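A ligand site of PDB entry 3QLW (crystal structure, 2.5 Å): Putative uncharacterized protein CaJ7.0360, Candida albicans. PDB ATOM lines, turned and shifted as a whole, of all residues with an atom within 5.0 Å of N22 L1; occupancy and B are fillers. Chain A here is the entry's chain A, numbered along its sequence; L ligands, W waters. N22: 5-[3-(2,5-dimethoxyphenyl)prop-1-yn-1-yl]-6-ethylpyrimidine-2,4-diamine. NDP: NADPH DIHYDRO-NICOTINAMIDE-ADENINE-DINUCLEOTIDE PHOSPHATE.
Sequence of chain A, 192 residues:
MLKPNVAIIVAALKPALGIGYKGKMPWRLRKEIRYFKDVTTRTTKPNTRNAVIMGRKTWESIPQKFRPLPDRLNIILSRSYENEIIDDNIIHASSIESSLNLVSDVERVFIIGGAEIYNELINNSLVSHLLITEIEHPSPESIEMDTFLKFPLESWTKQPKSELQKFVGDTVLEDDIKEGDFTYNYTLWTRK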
ATOM      1  N   ILE A   9       7.283  -4.670  -1.776  1.00  0.00           N
ATOM      2  CA  ILE A   9       6.478  -5.607  -2.560  1.00  0.00           C
ATOM      3  C   ILE A   9       6.058  -4.920  -3.862  1.00  0.00           C
ATOM      4  O   ILE A   9       5.540  -3.796  -3.837  1.00  0.00           O
ATOM      5  CB  ILE A   9       5.275  -6.155  -1.733  1.00  0.00           C
ATOM      6  CG1 ILE A   9       4.446  -7.161  -2.551  1.00  0.00           C
ATOM      7  CG2 ILE A   9       4.418  -5.020  -1.157  1.00  0.00           C
ATOM      8  CD1 ILE A   9       3.605  -8.098  -1.714  1.00  0.00           C
ATOM      9  N   VAL A  10       6.293  -5.593  -4.988  1.00  0.00           N
ATOM     10  CA  VAL A  10       6.034  -5.053  -6.328  1.00  0.00           C
ATOM     11  C   VAL A  10       5.907  -6.165  -7.370  1.00  0.00           C
ATOM     12  O   VAL A  10       6.487  -7.245  -7.213  1.00  0.00           O
ATOM     13  CB  VAL A  10       7.151  -4.026  -6.766  1.00  0.00           C
ATOM     14  CG1 VAL A  10       8.534  -4.691  -6.834  1.00  0.00           C
ATOM     15  CG2 VAL A  10       6.794  -3.350  -8.081  1.00  0.00           C
ATOM     16  N   ALA A  11       5.135  -5.901  -8.424  1.00  0.00           N
ATOM     17  CA  ALA A  11       5.055  -6.768  -9.593  1.00  0.00           C
ATOM     18  C   ALA A  11       5.571  -6.035 -10.832  1.00  0.00           C
ATOM     19  O   ALA A  11       5.095  -4.948 -11.163  1.00  0.00           O
ATOM     20  CB  ALA A  11       3.626  -7.259  -9.798  1.00  0.00           C
ATOM     21  N   MET A  25      -1.658   0.654 -14.179  1.00  0.00           N
ATOM     22  CA  MET A  25      -1.041  -0.654 -14.164  1.00  0.00           C
ATOM     23  C   MET A  25      -1.311  -1.341 -15.502  1.00  0.00           C
ATOM     24  O   MET A  25      -2.454  -1.352 -15.971  1.00  0.00           O
ATOM     25  CB  MET A  25      -1.623  -1.483 -13.020  1.00  0.00           C
ATOM     26  CG  MET A  25      -0.643  -2.423 -12.373  1.00  0.00           C
ATOM     27  SD  MET A  25      -1.015  -2.643 -10.632  1.00  0.00           S
ATOM     28  CE  MET A  25      -0.482  -1.078  -9.949  1.00  0.00           C
ATOM     29  N   GLU A  32      -2.273 -12.543  -8.354  1.00  0.00           N
ATOM     30  CA  GLU A  32      -1.253 -11.632  -7.872  1.00  0.00           C
ATOM     31  C   GLU A  32      -1.842 -10.618  -6.880  1.00  0.00           C
ATOM     32  O   GLU A  32      -1.283 -10.396  -5.802  1.00  0.00           O
ATOM     33  CB  GLU A  32      -0.595 -10.911  -9.059  1.00  0.00           C
ATOM     34  CG  GLU A  32       0.854 -10.510  -8.851  1.00  0.00           C
ATOM     35  CD  GLU A  32       1.031  -9.442  -7.781  1.00  0.00           C
ATOM     36  OE1 GLU A  32       0.287  -8.433  -7.802  1.00  0.00           O
ATOM     37  OE2 GLU A  32       1.919  -9.612  -6.929  1.00  0.00           O
ATOM     38  N   ILE A  33      -2.968 -10.025  -7.261  1.00  0.00           N
ATOM     39  CA  ILE A  33      -3.742  -9.124  -6.399  1.00  0.00           C
ATOM     40  C   ILE A  33      -4.058  -9.796  -5.058  1.00  0.00           C
ATOM     41  O   ILE A  33      -3.907  -9.188  -3.989  1.00  0.00           O
ATOM     42  CB  ILE A  33      -5.052  -8.671  -7.117  1.00  0.00           C
ATOM     43  CG1 ILE A  33      -4.726  -7.665  -8.225  1.00  0.00           C
ATOM     44  CG2 ILE A  33      -6.060  -8.086  -6.127  1.00  0.00           C
ATOM     45  CD1 ILE A  33      -5.764  -7.599  -9.333  1.00  0.00           C
ATOM     46  N   PHE A  36      -0.874 -10.375  -3.018  1.00  0.00           N
ATOM     47  CA  PHE A  36      -0.574  -9.067  -2.427  1.00  0.00           C
ATOM     48  C   PHE A  36      -1.375  -8.814  -1.153  1.00  0.00           C
ATOM     49  O   PHE A  36      -0.815  -8.370  -0.149  1.00  0.00           O
ATOM     50  CB  PHE A  36      -0.842  -7.965  -3.469  1.00  0.00           C
ATOM     51  CG  PHE A  36      -0.768  -6.567  -2.922  1.00  0.00           C
ATOM     52  CD1 PHE A  36       0.462  -5.951  -2.725  1.00  0.00           C
ATOM     53  CD2 PHE A  36      -1.937  -5.866  -2.610  1.00  0.00           C
ATOM     54  CE1 PHE A  36       0.535  -4.663  -2.219  1.00  0.00           C
ATOM     55  CE2 PHE A  36      -1.871  -4.573  -2.111  1.00  0.00           C
ATOM     56  CZ  PHE A  36      -0.632  -3.971  -1.919  1.00  0.00           C
ATOM     57  N   THR A  58      -0.131   6.889  -5.749  1.00  0.00           N
ATOM     58  CA  THR A  58      -0.631   5.520  -5.662  1.00  0.00           C
ATOM     59  C   THR A  58      -1.910   5.463  -4.827  1.00  0.00           C
ATOM     60  O   THR A  58      -2.865   4.782  -5.199  1.00  0.00           O
ATOM     61  CB  THR A  58       0.449   4.558  -5.102  1.00  0.00           C
ATOM     62  OG1 THR A  58       1.584   4.554  -5.979  1.00  0.00           O
ATOM     63  CG2 THR A  58      -0.089   3.134  -4.981  1.00  0.00           C
ATOM     64  N   SER A  61      -4.821   6.605  -6.749  1.00  0.00           N
ATOM     65  CA  SER A  61      -5.190   5.645  -7.795  1.00  0.00           C
ATOM     66  C   SER A  61      -5.920   4.409  -7.273  1.00  0.00           C
ATOM     67  O   SER A  61      -6.502   3.665  -8.065  1.00  0.00           O
ATOM     68  CB  SER A  61      -3.945   5.240  -8.587  1.00  0.00           C
ATOM     69  OG  SER A  61      -3.478   6.323  -9.381  1.00  0.00           O
ATOM     70  N   ILE A  62      -5.868   4.186  -5.958  1.00  0.00           N
ATOM     71  CA  ILE A  62      -6.579   3.079  -5.341  1.00  0.00           C
ATOM     72  C   ILE A  62      -8.097   3.312  -5.442  1.00  0.00           C
ATOM     73  O   ILE A  62      -8.580   4.350  -5.011  1.00  0.00           O
ATOM     74  CB  ILE A  62      -6.160   2.863  -3.852  1.00  0.00           C
ATOM     75  CG1 ILE A  62      -4.685   2.480  -3.762  1.00  0.00           C
ATOM     76  CG2 ILE A  62      -7.036   1.787  -3.189  1.00  0.00           C
ATOM     77  CD1 ILE A  62      -4.142   2.447  -2.350  1.00  0.00           C
ATOM     78  N   PRO A  63      -8.826   2.350  -6.034  1.00  0.00           N
ATOM     79  CA  PRO A  63     -10.280   2.444  -6.174  1.00  0.00           C
ATOM     80  C   PRO A  63     -10.958   2.875  -4.872  1.00  0.00           C
ATOM     81  O   PRO A  63     -10.582   2.413  -3.786  1.00  0.00           O
ATOM     82  CB  PRO A  63     -10.693   1.028  -6.561  1.00  0.00           C
ATOM     83  CG  PRO A  63      -9.521   0.511  -7.309  1.00  0.00           C
ATOM     84  CD  PRO A  63      -8.311   1.118  -6.661  1.00  0.00           C
ATOM     85  N   LEU A  69      -6.874   0.632   2.340  1.00  0.00           N
ATOM     86  CA  LEU A  69      -6.774  -0.818   2.223  1.00  0.00           C
ATOM     87  C   LEU A  69      -7.059  -1.474   3.577  1.00  0.00           C
ATOM     88  O   LEU A  69      -6.343  -1.235   4.551  1.00  0.00           O
ATOM     89  CB  LEU A  69      -5.389  -1.230   1.691  1.00  0.00           C
ATOM     90  CG  LEU A  69      -4.973  -0.774   0.287  1.00  0.00           C
ATOM     91  CD1 LEU A  69      -3.502  -1.055   0.076  1.00  0.00           C
ATOM     92  CD2 LEU A  69      -5.811  -1.433  -0.807  1.00  0.00           C
ATOM     93  N   ILE A 111       6.264  -1.511   1.628  1.00  0.00           N
ATOM     94  CA  ILE A 111       6.287  -0.432   0.647  1.00  0.00           C
ATOM     95  C   ILE A 111       5.591  -0.941  -0.613  1.00  0.00           C
ATOM     96  O   ILE A 111       6.032  -1.930  -1.221  1.00  0.00           O
ATOM     97  CB  ILE A 111       7.720   0.050   0.349  1.00  0.00           C
ATOM     98  CG1 ILE A 111       8.333   0.687   1.607  1.00  0.00           C
ATOM     99  CG2 ILE A 111       7.740   1.033  -0.806  1.00  0.00           C
ATOM    100  CD1 ILE A 111       9.828   0.559   1.702  1.00  0.00           C
ATOM    101  N   ILE A 112       4.504  -0.282  -1.001  1.00  0.00           N
ATOM    102  CA  ILE A 112       3.636  -0.793  -2.053  1.00  0.00           C
ATOM    103  C   ILE A 112       3.598   0.085  -3.322  1.00  0.00           C
ATOM    104  O   ILE A 112       2.846  -0.212  -4.249  1.00  0.00           O
ATOM    105  CB  ILE A 112       2.200  -1.091  -1.533  1.00  0.00           C
ATOM    106  CG1 ILE A 112       1.436   0.194  -1.190  1.00  0.00           C
ATOM    107  CG2 ILE A 112       2.253  -2.044  -0.331  1.00  0.00           C
ATOM    108  CD1 ILE A 112      -0.076   0.006  -1.096  1.00  0.00           C
ATOM    109  N   GLY A 113       4.417   1.137  -3.357  1.00  0.00           N
ATOM    110  CA  GLY A 113       4.524   1.980  -4.544  1.00  0.00           C
ATOM    111  C   GLY A 113       4.337   3.468  -4.304  1.00  0.00           C
ATOM    112  O   GLY A 113       4.144   3.902  -3.172  1.00  0.00           O
ATOM    113  N   TYR A 118       9.483   3.611  -4.695  1.00  0.00           N
ATOM    114  CA  TYR A 118      10.330   2.415  -4.877  1.00  0.00           C
ATOM    115  C   TYR A 118      11.785   2.790  -5.133  1.00  0.00           C
ATOM    116  O   TYR A 118      12.682   2.357  -4.420  1.00  0.00           O
ATOM    117  CB  TYR A 118       9.837   1.568  -6.052  1.00  0.00           C
ATOM    118  CG  TYR A 118       8.589   0.739  -5.838  1.00  0.00           C
ATOM    119  CD1 TYR A 118       8.398   0.002  -4.653  1.00  0.00           C
ATOM    120  CD2 TYR A 118       7.623   0.640  -6.836  1.00  0.00           C
ATOM    121  CE1 TYR A 118       7.253  -0.775  -4.482  1.00  0.00           C
ATOM    122  CE2 TYR A 118       6.489  -0.128  -6.669  1.00  0.00           C
ATOM    123  CZ  TYR A 118       6.309  -0.834  -5.488  1.00  0.00           C
ATOM    124  OH  TYR A 118       5.174  -1.593  -5.349  1.00  0.00           O
ATOM    125  N   LEU A 131      10.057  -8.277  -2.169  1.00  0.00           N
ATOM    126  CA  LEU A 131       9.110  -9.275  -2.655  1.00  0.00           C
ATOM    127  C   LEU A 131       8.718  -8.911  -4.081  1.00  0.00           C
ATOM    128  O   LEU A 131       7.735  -8.203  -4.317  1.00  0.00           O
ATOM    129  CB  LEU A 131       7.874  -9.332  -1.746  1.00  0.00           C
ATOM    130  CG  LEU A 131       8.091  -9.962  -0.364  1.00  0.00           C
ATOM    131  CD1 LEU A 131       7.240  -9.273   0.693  1.00  0.00           C
ATOM    132  CD2 LEU A 131       7.796 -11.446  -0.393  1.00  0.00           C
ATOM    133  N   THR A 133       7.373  -9.837  -7.680  1.00  0.00           N
ATOM    134  CA  THR A 133       6.665 -10.728  -8.578  1.00  0.00           C
ATOM    135  C   THR A 133       7.224 -10.505  -9.983  1.00  0.00           C
ATOM    136  O   THR A 133       7.016  -9.451 -10.598  1.00  0.00           O
ATOM    137  CB  THR A 133       5.138 -10.486  -8.569  1.00  0.00           C
ATOM    138  OG1 THR A 133       4.644 -10.582  -7.238  1.00  0.00           O
ATOM    139  CG2 THR A 133       4.433 -11.499  -9.453  1.00  0.00           C
HETATM  140  C8  N22 L   1      -1.202  -4.997  -8.073  1.00  0.00           C
HETATM  141  C7  N22 L   1      -1.113  -5.299  -6.586  1.00  0.00           C
HETATM  142  C5  N22 L   1       0.347  -5.201  -6.100  1.00  0.00           C
HETATM  143  N4  N22 L   1       1.114  -6.380  -6.205  1.00  0.00           N
HETATM  144  C3  N22 L   1       2.444  -6.395  -5.790  1.00  0.00           C
HETATM  145  N8  N22 L   1       3.171  -7.506  -5.876  1.00  0.00           N
HETATM  146  N2  N22 L   1       3.020  -5.237  -5.271  1.00  0.00           N
HETATM  147  C1  N22 L   1       2.273  -4.063  -5.175  1.00  0.00           C
HETATM  148  N7  N22 L   1       2.856  -2.981  -4.678  1.00  0.00           N
HETATM  149  C6  N22 L   1       0.943  -4.048  -5.591  1.00  0.00           C
HETATM  150  C9  N22 L   1       0.205  -2.822  -5.461  1.00  0.00           C
HETATM  151  C10 N22 L   1      -0.389  -1.758  -5.343  1.00  0.00           C
HETATM  152  C11 N22 L   1      -1.125  -0.488  -5.210  1.00  0.00           C
HETATM  153  C13 N22 L   1      -2.595  -0.702  -5.589  1.00  0.00           C
HETATM  154  C18 N22 L   1      -3.293  -1.645  -4.841  1.00  0.00           C
HETATM  155  C17 N22 L   1      -4.631  -1.927  -5.098  1.00  0.00           C
HETATM  156  O2  N22 L   1      -5.291  -2.853  -4.345  1.00  0.00           O
HETATM  157  C4  N22 L   1      -4.937  -4.213  -4.691  1.00  0.00           C
HETATM  158  C16 N22 L   1      -5.293  -1.238  -6.121  1.00  0.00           C
HETATM  159  C15 N22 L   1      -4.596  -0.290  -6.881  1.00  0.00           C
HETATM  160  C14 N22 L   1      -3.255  -0.022  -6.623  1.00  0.00           C
HETATM  161  O10 N22 L   1      -2.563   0.916  -7.349  1.00  0.00           O
HETATM  162  C2  N22 L   1      -3.139   1.289  -8.616  1.00  0.00           C
HETATM  163  PA  NDP L   2       4.029   7.563  -6.329  1.00  0.00           P
HETATM  164  O1A NDP L   2       5.398   7.078  -6.056  1.00  0.00           O
HETATM  165  O2A NDP L   2       3.009   6.599  -5.862  1.00  0.00           O
HETATM  166  O5B NDP L   2       3.789   9.009  -5.666  1.00  0.00           O
HETATM  167  C5B NDP L   2       4.704  10.051  -5.881  1.00  0.00           C
HETATM  168  C4B NDP L   2       4.504  11.068  -4.761  1.00  0.00           C
HETATM  169  O4B NDP L   2       5.000  10.561  -3.536  1.00  0.00           O
HETATM  170  C3B NDP L   2       5.243  12.369  -5.002  1.00  0.00           C
HETATM  171  O3B NDP L   2       4.495  13.244  -5.807  1.00  0.00           O
HETATM  172  C2B NDP L   2       5.430  12.881  -3.592  1.00  0.00           C
HETATM  173  O2B NDP L   2       4.254  13.517  -3.131  1.00  0.00           O
HETATM  174  C1B NDP L   2       5.562  11.610  -2.770  1.00  0.00           C
HETATM  175  N9A NDP L   2       6.972  11.296  -2.448  1.00  0.00           N
HETATM  176  C8A NDP L   2       7.934  10.819  -3.305  1.00  0.00           C
HETATM  177  N7A NDP L   2       9.083  10.641  -2.614  1.00  0.00           N
HETATM  178  C5A NDP L   2       8.860  11.008  -1.326  1.00  0.00           C
HETATM  179  C6A NDP L   2       9.687  11.025  -0.196  1.00  0.00           C
HETATM  180  N6A NDP L   2      10.956  10.639  -0.292  1.00  0.00           N
HETATM  181  N1A NDP L   2       9.173  11.445   1.007  1.00  0.00           N
HETATM  182  C2A NDP L   2       7.848  11.847   1.094  1.00  0.00           C
HETATM  183  N3A NDP L   2       7.038  11.828  -0.021  1.00  0.00           N
HETATM  184  C4A NDP L   2       7.533  11.413  -1.214  1.00  0.00           C
HETATM  185  O3  NDP L   2       3.826   7.864  -7.898  1.00  0.00           O
HETATM  186  PN  NDP L   2       4.675   7.436  -9.188  1.00  0.00           P
HETATM  187  O1N NDP L   2       4.139   8.180 -10.351  1.00  0.00           O
HETATM  188  O2N NDP L   2       6.109   7.532  -8.853  1.00  0.00           O
HETATM  189  O5D NDP L   2       4.309   5.884  -9.355  1.00  0.00           O
HETATM  190  C5D NDP L   2       3.003   5.499  -9.742  1.00  0.00           C
HETATM  191  C4D NDP L   2       3.092   4.439 -10.838  1.00  0.00           C
HETATM  192  O4D NDP L   2       3.566   3.226 -10.290  1.00  0.00           O
HETATM  193  C3D NDP L   2       1.737   4.151 -11.460  1.00  0.00           C
HETATM  194  O3D NDP L   2       1.891   4.038 -12.854  1.00  0.00           O
HETATM  195  C2D NDP L   2       1.336   2.811 -10.886  1.00  0.00           C
HETATM  196  O2D NDP L   2       0.588   2.052 -11.816  1.00  0.00           O
HETATM  197  C1D NDP L   2       2.677   2.160 -10.600  1.00  0.00           C
HETATM  198  N1N NDP L   2       2.627   1.167  -9.509  1.00  0.00           N
HETATM  199  C2N NDP L   2       2.963  -0.123  -9.805  1.00  0.00           C
HETATM  200  C3N NDP L   2       2.943  -1.113  -8.820  1.00  0.00           C
HETATM  201  C7N NDP L   2       3.221  -2.545  -9.192  1.00  0.00           C
HETATM  202  O7N NDP L   2       3.444  -3.491  -8.173  1.00  0.00           O
HETATM  203  N7N NDP L   2       3.254  -2.886 -10.481  1.00  0.00           N
HETATM  204  C4N NDP L   2       2.577  -0.769  -7.521  1.00  0.00           C
HETATM  205  C5N NDP L   2       2.249   0.560  -7.218  1.00  0.00           C
HETATM  206  C6N NDP L   2       2.277   1.519  -8.223  1.00  0.00           C
HETATM  207  P2B NDP L   2       4.020  15.103  -3.254  1.00  0.00           P
HETATM  208  O1X NDP L   2       2.612  15.397  -2.781  1.00  0.00           O
HETATM  209  O2X NDP L   2       5.018  15.824  -2.390  1.00  0.00           O
HETATM  210  O3X NDP L   2       4.133  15.522  -4.702  1.00  0.00           O
HETATM  211  O   HOH W   1       0.059  -7.273 -10.291  1.00  0.00           O
HETATM  212  O   HOH W   2       5.492  -9.485  -4.857  1.00  0.00           O
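The side-chain carboxylate (OE2) of Glu 32 lies within hydrogen-bond range of a nitrogen (N8) of N22 L1 (2.7 Å). OH of Tyr 118 is in hydrogen-bond range of N7 of N22 L1, 2.8 Å away. A nitrogen (N7) of N22 L1 sits at hydrogen-bond distance from the backbone carbonyl oxygen (O) of Ile 112 (2.8 Å). The backbone carbonyl oxygen of Ile 9 sits at hydrogen-bond distance from a nitrogen (N7) of N22 L1, 2.9 Å away. The backbone NH of Val 10 sits close to a nitrogen (N2) of N22 L1. The backbone NH of Ala 11 is in hydrogen-bond range of an oxygen (O7N) of NDP L2. The backbone carbonyl oxygen of Ala 11 sits at hydrogen-bond distance from a nitrogen (N7N) of NDP L2. The backbone NH of Thr 58 sits at hydrogen-bond distance from an oxygen (O2A) of NDP L2, at 3.2 Å. The side-chain hydroxyl of Thr 58 sits at hydrogen-bond distance from an oxygen (O2A) of NDP L2 (2.5 Å).
The side-chain carboxylate of Glu 32 is in hydrogen-bond range of the side-chain hydroxyl of Thr 133. The side-chain hydroxyl (OH) of Tyr 118 sits at hydrogen-bond distance from the backbone carbonyl oxygen (O) of Ile 112, at 2.9 Å. The backbone carbonyl oxygen of Ile 9 lies within hydrogen-bond range of the side-chain hydroxyl of Tyr 118. OH of Tyr 118 is in hydrogen-bond range of N of Gly 113, 3.5 Å away. O of Ile 111 is in hydrogen-bond range of N of Ile 9 (3.1 Å). N of Thr 133 is in hydrogen-bond range of O of Val 10, 2.8 Å away. The backbone NH (N) of Val 10 lies within hydrogen-bond range of the backbone carbonyl oxygen (O) of Leu 131, at 3.1 Å.
Ala 11 touches N22 L1 (N to N8, 3.6 Å). Met 25 touches N22 L1. CE1 of Phe 36 touches C6 of N22 L1, at 3.5 Å. Thr 58 touches N22 L1. CD of Pro 63 touches C16 of N22 L1, at 3.9 Å. CD2 of Leu 69 touches O2 of N22 L1, at 3.8 Å. Thr 133 touches N22 L1 (OG1 to N8, 3.7 Å). Hydrophobic or aromatic side chains within 4 Å of N22 L1: Ile 9, Ala 11, Met 25, Phe 36, Pro 63, Leu 69 and Ile 112.
Water W2 lies within hydrogen-bond range of the backbone carbonyl oxygen (O) of Leu 131 (2.6 Å), the side-chain hydroxyl (OG1) of Thr 133 (2.8 Å), a nitrogen (N8) of N22 L1 (3.2 Å) and the backbone carbonyl oxygen (O) of Val 10 (3.4 Å).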
